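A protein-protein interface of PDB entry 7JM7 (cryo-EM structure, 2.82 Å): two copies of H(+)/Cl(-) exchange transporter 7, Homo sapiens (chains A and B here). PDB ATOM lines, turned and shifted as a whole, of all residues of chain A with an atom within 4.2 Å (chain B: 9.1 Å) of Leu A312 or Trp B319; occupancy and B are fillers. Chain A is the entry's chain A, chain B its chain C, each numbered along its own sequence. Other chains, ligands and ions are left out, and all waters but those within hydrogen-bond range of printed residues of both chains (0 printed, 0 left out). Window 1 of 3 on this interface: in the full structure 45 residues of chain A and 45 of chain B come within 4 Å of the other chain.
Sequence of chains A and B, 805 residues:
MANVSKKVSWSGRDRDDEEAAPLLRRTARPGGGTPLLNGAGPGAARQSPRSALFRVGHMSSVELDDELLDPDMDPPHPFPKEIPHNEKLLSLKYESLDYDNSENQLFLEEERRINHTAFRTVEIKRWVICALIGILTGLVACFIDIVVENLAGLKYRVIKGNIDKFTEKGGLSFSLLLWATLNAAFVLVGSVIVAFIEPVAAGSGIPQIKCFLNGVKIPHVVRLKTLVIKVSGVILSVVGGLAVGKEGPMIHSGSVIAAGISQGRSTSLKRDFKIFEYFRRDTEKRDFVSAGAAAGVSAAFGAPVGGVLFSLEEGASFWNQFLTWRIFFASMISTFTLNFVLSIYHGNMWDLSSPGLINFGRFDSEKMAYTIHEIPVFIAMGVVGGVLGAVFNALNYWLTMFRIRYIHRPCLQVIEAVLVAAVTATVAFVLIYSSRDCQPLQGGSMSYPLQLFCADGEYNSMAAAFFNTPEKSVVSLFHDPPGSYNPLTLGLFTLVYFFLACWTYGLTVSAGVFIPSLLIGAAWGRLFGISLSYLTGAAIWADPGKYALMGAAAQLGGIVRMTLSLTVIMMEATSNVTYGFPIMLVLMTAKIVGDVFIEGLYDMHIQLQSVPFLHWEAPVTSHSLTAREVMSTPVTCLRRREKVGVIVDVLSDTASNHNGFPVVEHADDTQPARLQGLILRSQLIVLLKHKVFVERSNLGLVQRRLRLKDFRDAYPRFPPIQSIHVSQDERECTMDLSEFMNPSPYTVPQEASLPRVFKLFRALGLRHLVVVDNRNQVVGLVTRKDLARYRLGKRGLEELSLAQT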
ATOM      1  N   VAL A 308      32.221  -7.566   3.508  1.00  0.00           N
ATOM      2  CA  VAL A 308      31.876  -6.316   4.177  1.00  0.00           C
ATOM      3  C   VAL A 308      31.744  -6.546   5.676  1.00  0.00           C
ATOM      4  O   VAL A 308      32.258  -5.769   6.489  1.00  0.00           O
ATOM      5  CB  VAL A 308      30.583  -5.731   3.579  1.00  0.00           C
ATOM      6  CG1 VAL A 308      30.153  -4.494   4.342  1.00  0.00           C
ATOM      7  CG2 VAL A 308      30.774  -5.404   2.111  1.00  0.00           C
ATOM      8  N   LEU A 309      31.060  -7.623   6.064  1.00  0.00           N
ATOM      9  CA  LEU A 309      30.895  -7.925   7.481  1.00  0.00           C
ATOM     10  C   LEU A 309      32.226  -8.266   8.136  1.00  0.00           C
ATOM     11  O   LEU A 309      32.470  -7.887   9.285  1.00  0.00           O
ATOM     12  CB  LEU A 309      29.903  -9.070   7.661  1.00  0.00           C
ATOM     13  CG  LEU A 309      28.437  -8.746   7.367  1.00  0.00           C
ATOM     14  CD1 LEU A 309      27.606 -10.005   7.451  1.00  0.00           C
ATOM     15  CD2 LEU A 309      27.901  -7.690   8.316  1.00  0.00           C
ATOM     16  N   PHE A 310      33.095  -8.992   7.431  1.00  0.00           N
ATOM     17  CA  PHE A 310      34.417  -9.294   7.969  1.00  0.00           C
ATOM     18  C   PHE A 310      35.177  -8.011   8.279  1.00  0.00           C
ATOM     19  O   PHE A 310      35.733  -7.846   9.374  1.00  0.00           O
ATOM     20  CB  PHE A 310      35.191 -10.154   6.966  1.00  0.00           C
ATOM     21  CG  PHE A 310      36.648 -10.315   7.292  1.00  0.00           C
ATOM     22  CD1 PHE A 310      37.082 -11.366   8.076  1.00  0.00           C
ATOM     23  CD2 PHE A 310      37.585  -9.421   6.804  1.00  0.00           C
ATOM     24  CE1 PHE A 310      38.419 -11.518   8.374  1.00  0.00           C
ATOM     25  CE2 PHE A 310      38.921  -9.567   7.102  1.00  0.00           C
ATOM     26  CZ  PHE A 310      39.339 -10.618   7.887  1.00  0.00           C
ATOM     27  N   SER A 311      35.204  -7.087   7.319  1.00  0.00           N
ATOM     28  CA  SER A 311      35.905  -5.825   7.526  1.00  0.00           C
ATOM     29  C   SER A 311      35.280  -5.026   8.662  1.00  0.00           C
ATOM     30  O   SER A 311      35.995  -4.430   9.476  1.00  0.00           O
ATOM     31  CB  SER A 311      35.906  -5.014   6.233  1.00  0.00           C
ATOM     32  OG  SER A 311      34.626  -4.470   5.974  1.00  0.00           O
ATOM     33  N   LEU A 312      33.948  -4.999   8.732  1.00  0.00           N
ATOM     34  CA  LEU A 312      33.280  -4.264   9.802  1.00  0.00           C
ATOM     35  C   LEU A 312      33.620  -4.845  11.168  1.00  0.00           C
ATOM     36  O   LEU A 312      33.871  -4.104  12.124  1.00  0.00           O
ATOM     37  CB  LEU A 312      31.769  -4.280   9.581  1.00  0.00           C
ATOM     38  CG  LEU A 312      31.227  -3.467   8.409  1.00  0.00           C
ATOM     39  CD1 LEU A 312      29.727  -3.669   8.293  1.00  0.00           C
ATOM     40  CD2 LEU A 312      31.559  -2.003   8.562  1.00  0.00           C
ATOM     41  N   GLU A 313      33.622  -6.174  11.280  1.00  0.00           N
ATOM     42  CA  GLU A 313      33.956  -6.816  12.546  1.00  0.00           C
ATOM     43  C   GLU A 313      35.388  -6.507  12.955  1.00  0.00           C
ATOM     44  O   GLU A 313      35.659  -6.184  14.117  1.00  0.00           O
ATOM     45  CB  GLU A 313      33.757  -8.325  12.432  1.00  0.00           C
ATOM     46  CG  GLU A 313      32.321  -8.761  12.294  1.00  0.00           C
ATOM     47  CD  GLU A 313      32.178 -10.265  12.278  1.00  0.00           C
ATOM     48  OE1 GLU A 313      33.107 -10.957  12.742  1.00  0.00           O
ATOM     49  OE2 GLU A 313      31.143 -10.755  11.791  1.00  0.00           O
ATOM     50  N   GLU A 314      36.327  -6.612  12.012  1.00  0.00           N
ATOM     51  CA  GLU A 314      37.723  -6.380  12.364  1.00  0.00           C
ATOM     52  C   GLU A 314      37.964  -4.923  12.741  1.00  0.00           C
ATOM     53  O   GLU A 314      38.666  -4.640  13.718  1.00  0.00           O
ATOM     54  CB  GLU A 314      38.636  -6.801  11.213  1.00  0.00           C
ATOM     55  CG  GLU A 314      38.593  -8.289  10.879  1.00  0.00           C
ATOM     56  CD  GLU A 314      38.467  -9.177  12.101  1.00  0.00           C
ATOM     57  OE1 GLU A 314      39.220  -8.964  13.073  1.00  0.00           O
ATOM     58  OE2 GLU A 314      37.615 -10.089  12.089  1.00  0.00           O
ATOM     59  N   GLY A 315      37.394  -3.985  11.983  1.00  0.00           N
ATOM     60  CA  GLY A 315      37.521  -2.585  12.351  1.00  0.00           C
ATOM     61  C   GLY A 315      36.843  -2.268  13.671  1.00  0.00           C
ATOM     62  O   GLY A 315      37.425  -1.616  14.541  1.00  0.00           O
ATOM     63  N   ALA A 316      35.606  -2.737  13.839  1.00  0.00           N
ATOM     64  CA  ALA A 316      34.853  -2.561  15.079  1.00  0.00           C
ATOM     65  C   ALA A 316      34.870  -1.104  15.530  1.00  0.00           C
ATOM     66  O   ALA A 316      35.229  -0.779  16.664  1.00  0.00           O
ATOM     67  CB  ALA A 316      35.394  -3.477  16.175  1.00  0.00           C
ATOM     68  N   SER A 317      34.462  -0.219  14.630  1.00  0.00           N
ATOM     69  CA  SER A 317      34.526   1.218  14.845  1.00  0.00           C
ATOM     70  C   SER A 317      33.126   1.822  14.823  1.00  0.00           C
ATOM     71  O   SER A 317      32.115   1.121  14.740  1.00  0.00           O
ATOM     72  CB  SER A 317      35.407   1.883  13.786  1.00  0.00           C
ATOM     73  OG  SER A 317      34.682   2.094  12.588  1.00  0.00           O
ATOM     74  N   THR A 324      30.993   2.132   4.354  1.00  0.00           N
ATOM     75  CA  THR A 324      30.378   0.828   4.135  1.00  0.00           C
ATOM     76  C   THR A 324      29.869   0.699   2.705  1.00  0.00           C
ATOM     77  O   THR A 324      30.019  -0.356   2.074  1.00  0.00           O
ATOM     78  CB  THR A 324      29.247   0.614   5.135  1.00  0.00           C
ATOM     79  OG1 THR A 324      29.682   1.017   6.439  1.00  0.00           O
ATOM     80  CG2 THR A 324      28.844  -0.845   5.179  1.00  0.00           C
ATOM     81  N   TYR B  99      20.139   6.644  26.139  1.00  0.00           N
ATOM     82  CA  TYR B  99      20.980   5.500  25.807  1.00  0.00           C
ATOM     83  C   TYR B  99      22.282   5.509  26.596  1.00  0.00           C
ATOM     84  O   TYR B  99      22.866   4.446  26.837  1.00  0.00           O
ATOM     85  CB  TYR B  99      21.272   5.475  24.306  1.00  0.00           C
ATOM     86  CG  TYR B  99      21.874   4.172  23.833  1.00  0.00           C
ATOM     87  CD1 TYR B  99      21.170   2.983  23.941  1.00  0.00           C
ATOM     88  CD2 TYR B  99      23.143   4.130  23.282  1.00  0.00           C
ATOM     89  CE1 TYR B  99      21.712   1.792  23.517  1.00  0.00           C
ATOM     90  CE2 TYR B  99      23.695   2.941  22.852  1.00  0.00           C
ATOM     91  CZ  TYR B  99      22.974   1.774  22.973  1.00  0.00           C
ATOM     92  OH  TYR B  99      23.516   0.584  22.547  1.00  0.00           O
ATOM     93  N   VAL B 308      19.138  -6.861   9.532  1.00  0.00           N
ATOM     94  CA  VAL B 308      20.266  -6.520  10.392  1.00  0.00           C
ATOM     95  C   VAL B 308      20.917  -5.230   9.914  1.00  0.00           C
ATOM     96  O   VAL B 308      21.225  -4.335  10.710  1.00  0.00           O
ATOM     97  CB  VAL B 308      21.277  -7.681  10.431  1.00  0.00           C
ATOM     98  CG1 VAL B 308      22.505  -7.295  11.231  1.00  0.00           C
ATOM     99  CG2 VAL B 308      20.637  -8.924  11.017  1.00  0.00           C
ATOM    100  N   LEU B 309      21.128  -5.110   8.603  1.00  0.00           N
ATOM    101  CA  LEU B 309      21.736  -3.903   8.057  1.00  0.00           C
ATOM    102  C   LEU B 309      20.832  -2.691   8.243  1.00  0.00           C
ATOM    103  O   LEU B 309      21.315  -1.590   8.519  1.00  0.00           O
ATOM    104  CB  LEU B 309      22.066  -4.101   6.580  1.00  0.00           C
ATOM    105  CG  LEU B 309      23.223  -5.050   6.268  1.00  0.00           C
ATOM    106  CD1 LEU B 309      23.333  -5.253   4.776  1.00  0.00           C
ATOM    107  CD2 LEU B 309      24.532  -4.532   6.834  1.00  0.00           C
ATOM    108  N   LEU B 312      21.239  -1.638  11.808  1.00  0.00           N
ATOM    109  CA  LEU B 312      22.557  -1.048  12.014  1.00  0.00           C
ATOM    110  C   LEU B 312      22.622   0.366  11.449  1.00  0.00           C
ATOM    111  O   LEU B 312      23.181   1.270  12.079  1.00  0.00           O
ATOM    112  CB  LEU B 312      23.627  -1.926  11.370  1.00  0.00           C
ATOM    113  CG  LEU B 312      23.908  -3.277  12.023  1.00  0.00           C
ATOM    114  CD1 LEU B 312      24.931  -4.042  11.205  1.00  0.00           C
ATOM    115  CD2 LEU B 312      24.382  -3.103  13.446  1.00  0.00           C
ATOM    116  N   GLU B 313      22.067   0.570  10.255  1.00  0.00           N
ATOM    117  CA  GLU B 313      22.066   1.896   9.648  1.00  0.00           C
ATOM    118  C   GLU B 313      21.272   2.883  10.490  1.00  0.00           C
ATOM    119  O   GLU B 313      21.714   4.012  10.727  1.00  0.00           O
ATOM    120  CB  GLU B 313      21.486   1.822   8.238  1.00  0.00           C
ATOM    121  CG  GLU B 313      22.344   1.084   7.242  1.00  0.00           C
ATOM    122  CD  GLU B 313      21.764   1.124   5.849  1.00  0.00           C
ATOM    123  OE1 GLU B 313      20.930   2.010   5.573  1.00  0.00           O
ATOM    124  OE2 GLU B 313      22.134   0.261   5.030  1.00  0.00           O
ATOM    125  N   GLY B 315      20.436   2.729  13.746  1.00  0.00           N
ATOM    126  CA  GLY B 315      21.135   3.003  14.991  1.00  0.00           C
ATOM    127  C   GLY B 315      22.379   3.845  14.784  1.00  0.00           C
ATOM    128  O   GLY B 315      22.603   4.830  15.491  1.00  0.00           O
ATOM    129  N   ALA B 316      23.200   3.472  13.804  1.00  0.00           N
ATOM    130  CA  ALA B 316      24.405   4.220  13.449  1.00  0.00           C
ATOM    131  C   ALA B 316      25.252   4.515  14.685  1.00  0.00           C
ATOM    132  O   ALA B 316      25.614   5.658  14.966  1.00  0.00           O
ATOM    133  CB  ALA B 316      24.047   5.509  12.715  1.00  0.00           C
ATOM    134  N   SER B 317      25.578   3.461  15.422  1.00  0.00           N
ATOM    135  CA  SER B 317      26.276   3.568  16.694  1.00  0.00           C
ATOM    136  C   SER B 317      27.628   2.868  16.620  1.00  0.00           C
ATOM    137  O   SER B 317      28.060   2.392  15.568  1.00  0.00           O
ATOM    138  CB  SER B 317      25.432   2.974  17.824  1.00  0.00           C
ATOM    139  OG  SER B 317      25.569   1.565  17.867  1.00  0.00           O
ATOM    140  N   PHE B 318      28.300   2.826  17.767  1.00  0.00           N
ATOM    141  CA  PHE B 318      29.528   2.059  17.897  1.00  0.00           C
ATOM    142  C   PHE B 318      29.256   0.592  17.601  1.00  0.00           C
ATOM    143  O   PHE B 318      28.217   0.048  17.982  1.00  0.00           O
ATOM    144  CB  PHE B 318      30.092   2.212  19.308  1.00  0.00           C
ATOM    145  CG  PHE B 318      29.179   1.687  20.378  1.00  0.00           C
ATOM    146  CD1 PHE B 318      28.242   2.513  20.977  1.00  0.00           C
ATOM    147  CD2 PHE B 318      29.247   0.363  20.777  1.00  0.00           C
ATOM    148  CE1 PHE B 318      27.399   2.029  21.954  1.00  0.00           C
ATOM    149  CE2 PHE B 318      28.403  -0.126  21.750  1.00  0.00           C
ATOM    150  CZ  PHE B 318      27.477   0.708  22.339  1.00  0.00           C
ATOM    151  N   TRP B 319      30.195  -0.053  16.915  1.00  0.00           N
ATOM    152  CA  TRP B 319      30.023  -1.459  16.585  1.00  0.00           C
ATOM    153  C   TRP B 319      29.902  -2.292  17.854  1.00  0.00           C
ATOM    154  O   TRP B 319      30.713  -2.167  18.775  1.00  0.00           O
ATOM    155  CB  TRP B 319      31.193  -1.958  15.740  1.00  0.00           C
ATOM    156  CG  TRP B 319      31.082  -3.407  15.407  1.00  0.00           C
ATOM    157  CD1 TRP B 319      31.627  -4.450  16.094  1.00  0.00           C
ATOM    158  CD2 TRP B 319      30.368  -3.980  14.309  1.00  0.00           C
ATOM    159  NE1 TRP B 319      31.299  -5.637  15.492  1.00  0.00           N
ATOM    160  CE2 TRP B 319      30.526  -5.376  14.392  1.00  0.00           C
ATOM    161  CE3 TRP B 319      29.612  -3.449  13.261  1.00  0.00           C
ATOM    162  CZ2 TRP B 319      29.958  -6.245  13.470  1.00  0.00           C
ATOM    163  CZ3 TRP B 319      29.050  -4.311  12.350  1.00  0.00           C
ATOM    164  CH2 TRP B 319      29.224  -5.694  12.457  1.00  0.00           C
ATOM    165  N   ASN B 320      28.881  -3.144  17.896  1.00  0.00           N
ATOM    166  CA  ASN B 320      28.663  -4.073  18.999  1.00  0.00           C
ATOM    167  C   ASN B 320      28.515  -5.465  18.408  1.00  0.00           C
ATOM    168  O   ASN B 320      27.568  -5.731  17.663  1.00  0.00           O
ATOM    169  CB  ASN B 320      27.431  -3.685  19.814  1.00  0.00           C
ATOM    170  CG  ASN B 320      27.431  -4.299  21.196  1.00  0.00           C
ATOM    171  OD1 ASN B 320      28.201  -5.213  21.483  1.00  0.00           O
ATOM    172  ND2 ASN B 320      26.563  -3.798  22.062  1.00  0.00           N
ATOM    173  N   GLN B 321      29.457  -6.349  18.734  1.00  0.00           N
ATOM    174  CA  GLN B 321      29.472  -7.677  18.131  1.00  0.00           C
ATOM    175  C   GLN B 321      28.330  -8.539  18.655  1.00  0.00           C
ATOM    176  O   GLN B 321      27.608  -9.175  17.877  1.00  0.00           O
ATOM    177  CB  GLN B 321      30.821  -8.342  18.402  1.00  0.00           C
ATOM    178  CG  GLN B 321      31.032  -9.643  17.674  1.00  0.00           C
ATOM    179  CD  GLN B 321      31.191  -9.453  16.184  1.00  0.00           C
ATOM    180  OE1 GLN B 321      31.128  -8.334  15.676  1.00  0.00           O
ATOM    181  NE2 GLN B 321      31.391 -10.550  15.470  1.00  0.00           N
ATOM    182  N   PHE B 322      28.146  -8.564  19.975  1.00  0.00           N
ATOM    183  CA  PHE B 322      27.147  -9.445  20.567  1.00  0.00           C
ATOM    184  C   PHE B 322      25.734  -8.991  20.222  1.00  0.00           C
ATOM    185  O   PHE B 322      24.853  -9.821  19.965  1.00  0.00           O
ATOM    186  CB  PHE B 322      27.354  -9.507  22.079  1.00  0.00           C
ATOM    187  CG  PHE B 322      28.743  -9.917  22.479  1.00  0.00           C
ATOM    188  CD1 PHE B 322      29.738  -8.970  22.643  1.00  0.00           C
ATOM    189  CD2 PHE B 322      29.054 -11.250  22.686  1.00  0.00           C
ATOM    190  CE1 PHE B 322      31.017  -9.343  23.004  1.00  0.00           C
ATOM    191  CE2 PHE B 322      30.332 -11.628  23.049  1.00  0.00           C
ATOM    192  CZ  PHE B 322      31.314 -10.672  23.209  1.00  0.00           C
ATOM    193  N   LEU B 323      25.498  -7.680  20.203  1.00  0.00           N
ATOM    194  CA  LEU B 323      24.190  -7.175  19.806  1.00  0.00           C
ATOM    195  C   LEU B 323      23.878  -7.535  18.360  1.00  0.00           C
ATOM    196  O   LEU B 323      22.742  -7.897  18.033  1.00  0.00           O
ATOM    197  CB  LEU B 323      24.130  -5.663  20.003  1.00  0.00           C
ATOM    198  CG  LEU B 323      22.809  -4.999  19.623  1.00  0.00           C
ATOM    199  CD1 LEU B 323      21.697  -5.505  20.513  1.00  0.00           C
ATOM    200  CD2 LEU B 323      22.927  -3.494  19.713  1.00  0.00           C
ATOM    201  N   THR B 324      24.868  -7.422  17.475  1.00  0.00           N
ATOM    202  CA  THR B 324      24.658  -7.793  16.082  1.00  0.00           C
ATOM    203  C   THR B 324      24.372  -9.284  15.952  1.00  0.00           C
ATOM    204  O   THR B 324      23.501  -9.694  15.173  1.00  0.00           O
ATOM    205  CB  THR B 324      25.875  -7.399  15.252  1.00  0.00           C
ATOM    206  OG1 THR B 324      26.289  -6.075  15.612  1.00  0.00           O
ATOM    207  CG2 THR B 324      25.545  -7.428  13.775  1.00  0.00           C
ATOM    208  N   TRP B 325      25.093 -10.112  16.712  1.00  0.00           N
ATOM    209  CA  TRP B 325      24.794 -11.539  16.735  1.00  0.00           C
ATOM    210  C   TRP B 325      23.350 -11.782  17.151  1.00  0.00           C
ATOM    211  O   TRP B 325      22.641 -12.590  16.541  1.00  0.00           O
ATOM    212  CB  TRP B 325      25.739 -12.263  17.694  1.00  0.00           C
ATOM    213  CG  TRP B 325      27.154 -12.388  17.227  1.00  0.00           C
ATOM    214  CD1 TRP B 325      27.630 -12.179  15.967  1.00  0.00           C
ATOM    215  CD2 TRP B 325      28.281 -12.759  18.025  1.00  0.00           C
ATOM    216  NE1 TRP B 325      28.986 -12.398  15.931  1.00  0.00           N
ATOM    217  CE2 TRP B 325      29.409 -12.755  17.185  1.00  0.00           C
ATOM    218  CE3 TRP B 325      28.447 -13.095  19.372  1.00  0.00           C
ATOM    219  CZ2 TRP B 325      30.684 -13.071  17.644  1.00  0.00           C
ATOM    220  CZ3 TRP B 325      29.712 -13.409  19.827  1.00  0.00           C
ATOM    221  CH2 TRP B 325      30.814 -13.396  18.966  1.00  0.00           C
ATOM    222  N   ILE B 327      20.751  -9.735  16.997  1.00  0.00           N
ATOM    223  CA  ILE B 327      19.822  -9.267  15.971  1.00  0.00           C
ATOM    224  C   ILE B 327      19.735 -10.276  14.832  1.00  0.00           C
ATOM    225  O   ILE B 327      18.644 -10.585  14.332  1.00  0.00           O
ATOM    226  CB  ILE B 327      20.251  -7.877  15.462  1.00  0.00           C
ATOM    227  CG1 ILE B 327      20.187  -6.850  16.591  1.00  0.00           C
ATOM    228  CG2 ILE B 327      19.372  -7.438  14.311  1.00  0.00           C
ATOM    229  CD1 ILE B 327      20.989  -5.603  16.320  1.00  0.00           C
ATOM    230  N   LEU B 564      22.050   0.296   0.765  1.00  0.00           N
ATOM    231  CA  LEU B 564      22.769  -0.894   1.208  1.00  0.00           C
ATOM    232  C   LEU B 564      21.808  -1.985   1.668  1.00  0.00           C
ATOM    233  O   LEU B 564      21.781  -3.086   1.106  1.00  0.00           O
ATOM    234  CB  LEU B 564      23.741  -0.516   2.328  1.00  0.00           C
ATOM    235  CG  LEU B 564      24.684  -1.602   2.846  1.00  0.00           C
ATOM    236  CD1 LEU B 564      25.822  -1.820   1.875  1.00  0.00           C
ATOM    237  CD2 LEU B 564      25.213  -1.223   4.213  1.00  0.00           C
ATOM    238  N   ALA B 763      27.432   8.656  17.484  1.00  0.00           N
ATOM    239  CA  ALA B 763      27.970   7.324  17.724  1.00  0.00           C
ATOM    240  C   ALA B 763      27.631   6.825  19.120  1.00  0.00           C
ATOM    241  O   ALA B 763      27.223   5.670  19.290  1.00  0.00           O
ATOM    242  CB  ALA B 763      29.481   7.334  17.516  1.00  0.00           C
ATOM    243  N   LEU B 764      27.792   7.674  20.135  1.00  0.00           N
ATOM    244  CA  LEU B 764      27.595   7.229  21.507  1.00  0.00           C
ATOM    245  C   LEU B 764      26.141   7.287  21.953  1.00  0.00           C
ATOM    246  O   LEU B 764      25.835   6.831  23.060  1.00  0.00           O
ATOM    247  CB  LEU B 764      28.454   8.068  22.452  1.00  0.00           C
ATOM    248  CG  LEU B 764      29.894   7.588  22.624  1.00  0.00           C
ATOM    249  CD1 LEU B 764      30.741   8.686  23.224  1.00  0.00           C
ATOM    250  CD2 LEU B 764      29.946   6.344  23.484  1.00  0.00           C
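The backbone NH (N) of Trp B319 lies within hydrogen-bond range of the backbone carbonyl oxygen (O) of Ser A317, 3.1 Å away. The side-chain amide nitrogen (NE2) of Gln B321 sits at hydrogen-bond distance from the side-chain carboxylate (OE1) of Glu A313 (3.2 Å).
OE1 of Gln B321 sits at hydrogen-bond distance from NE1 of Trp B319, at 2.7 Å. The side-chain amide nitrogen (NE2) of Gln B321 sits close to the indole nitrogen (NE1) of Trp B325 (3.1 Å).
CZ3 of Trp B319 touches CB of Leu A312, at 3.9 Å. CG of Glu A313 touches CZ2 of Trp B319 (3.6 Å). Trp B319 touches Ala A316. CG2 of Thr A324 touches CD2 of Leu B564 (3.8 Å).
No residue of chain B comes within 4 Å of Ser A311. Of chain B, only Trp B319 comes within 4 Å of Leu A312. Of the printed residues of chain B, Glu A313 touches Trp B319 and Gln B321. No residue of chain B comes within 4 Å of Gly A315. Of chain B, only Trp B319 (3.8 Å) comes within 4 Å of Ala A316. Of the printed residues of chain B, Ser A317 touches Trp B319 (3.1 Å). Of the printed residues of chain B, Thr A324 touches Leu B564. Trp B319 touches four residues of chain A. Printed residues of chain A within 4 Å of Gln B321: Glu A313. Of the printed residues of chain A, Leu B564 touches Thr A324 (3.8 Å). The nearest residue of chain B that does not touch Leu A312 is Leu B309 (5.5 Å).
Of the 20 printed residues of chain B, 3 touch a printed residue of chain A. Hydrophobic or aromatic side chains of chain B that line the printed part of chain A: Trp B319 and Leu B564. Of the 11 printed residues of chain A, 5 touch a printed residue of chain B. Printed residues of chain A that touch a printed residue of chain B: Leu A312, Glu A313, Ala A316, Ser A317 and Thr A324. Hydrophobic or aromatic side chains of chain A that line the printed part of chain B: Leu A312 and Ala A316.
Positions printed for both chains: 308, 309, 312, 313, 315, 316, 317 and 324. Of the 6 pairs that touch across the chains among the printed residues, none has its exchanged pair printed and touching as well.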
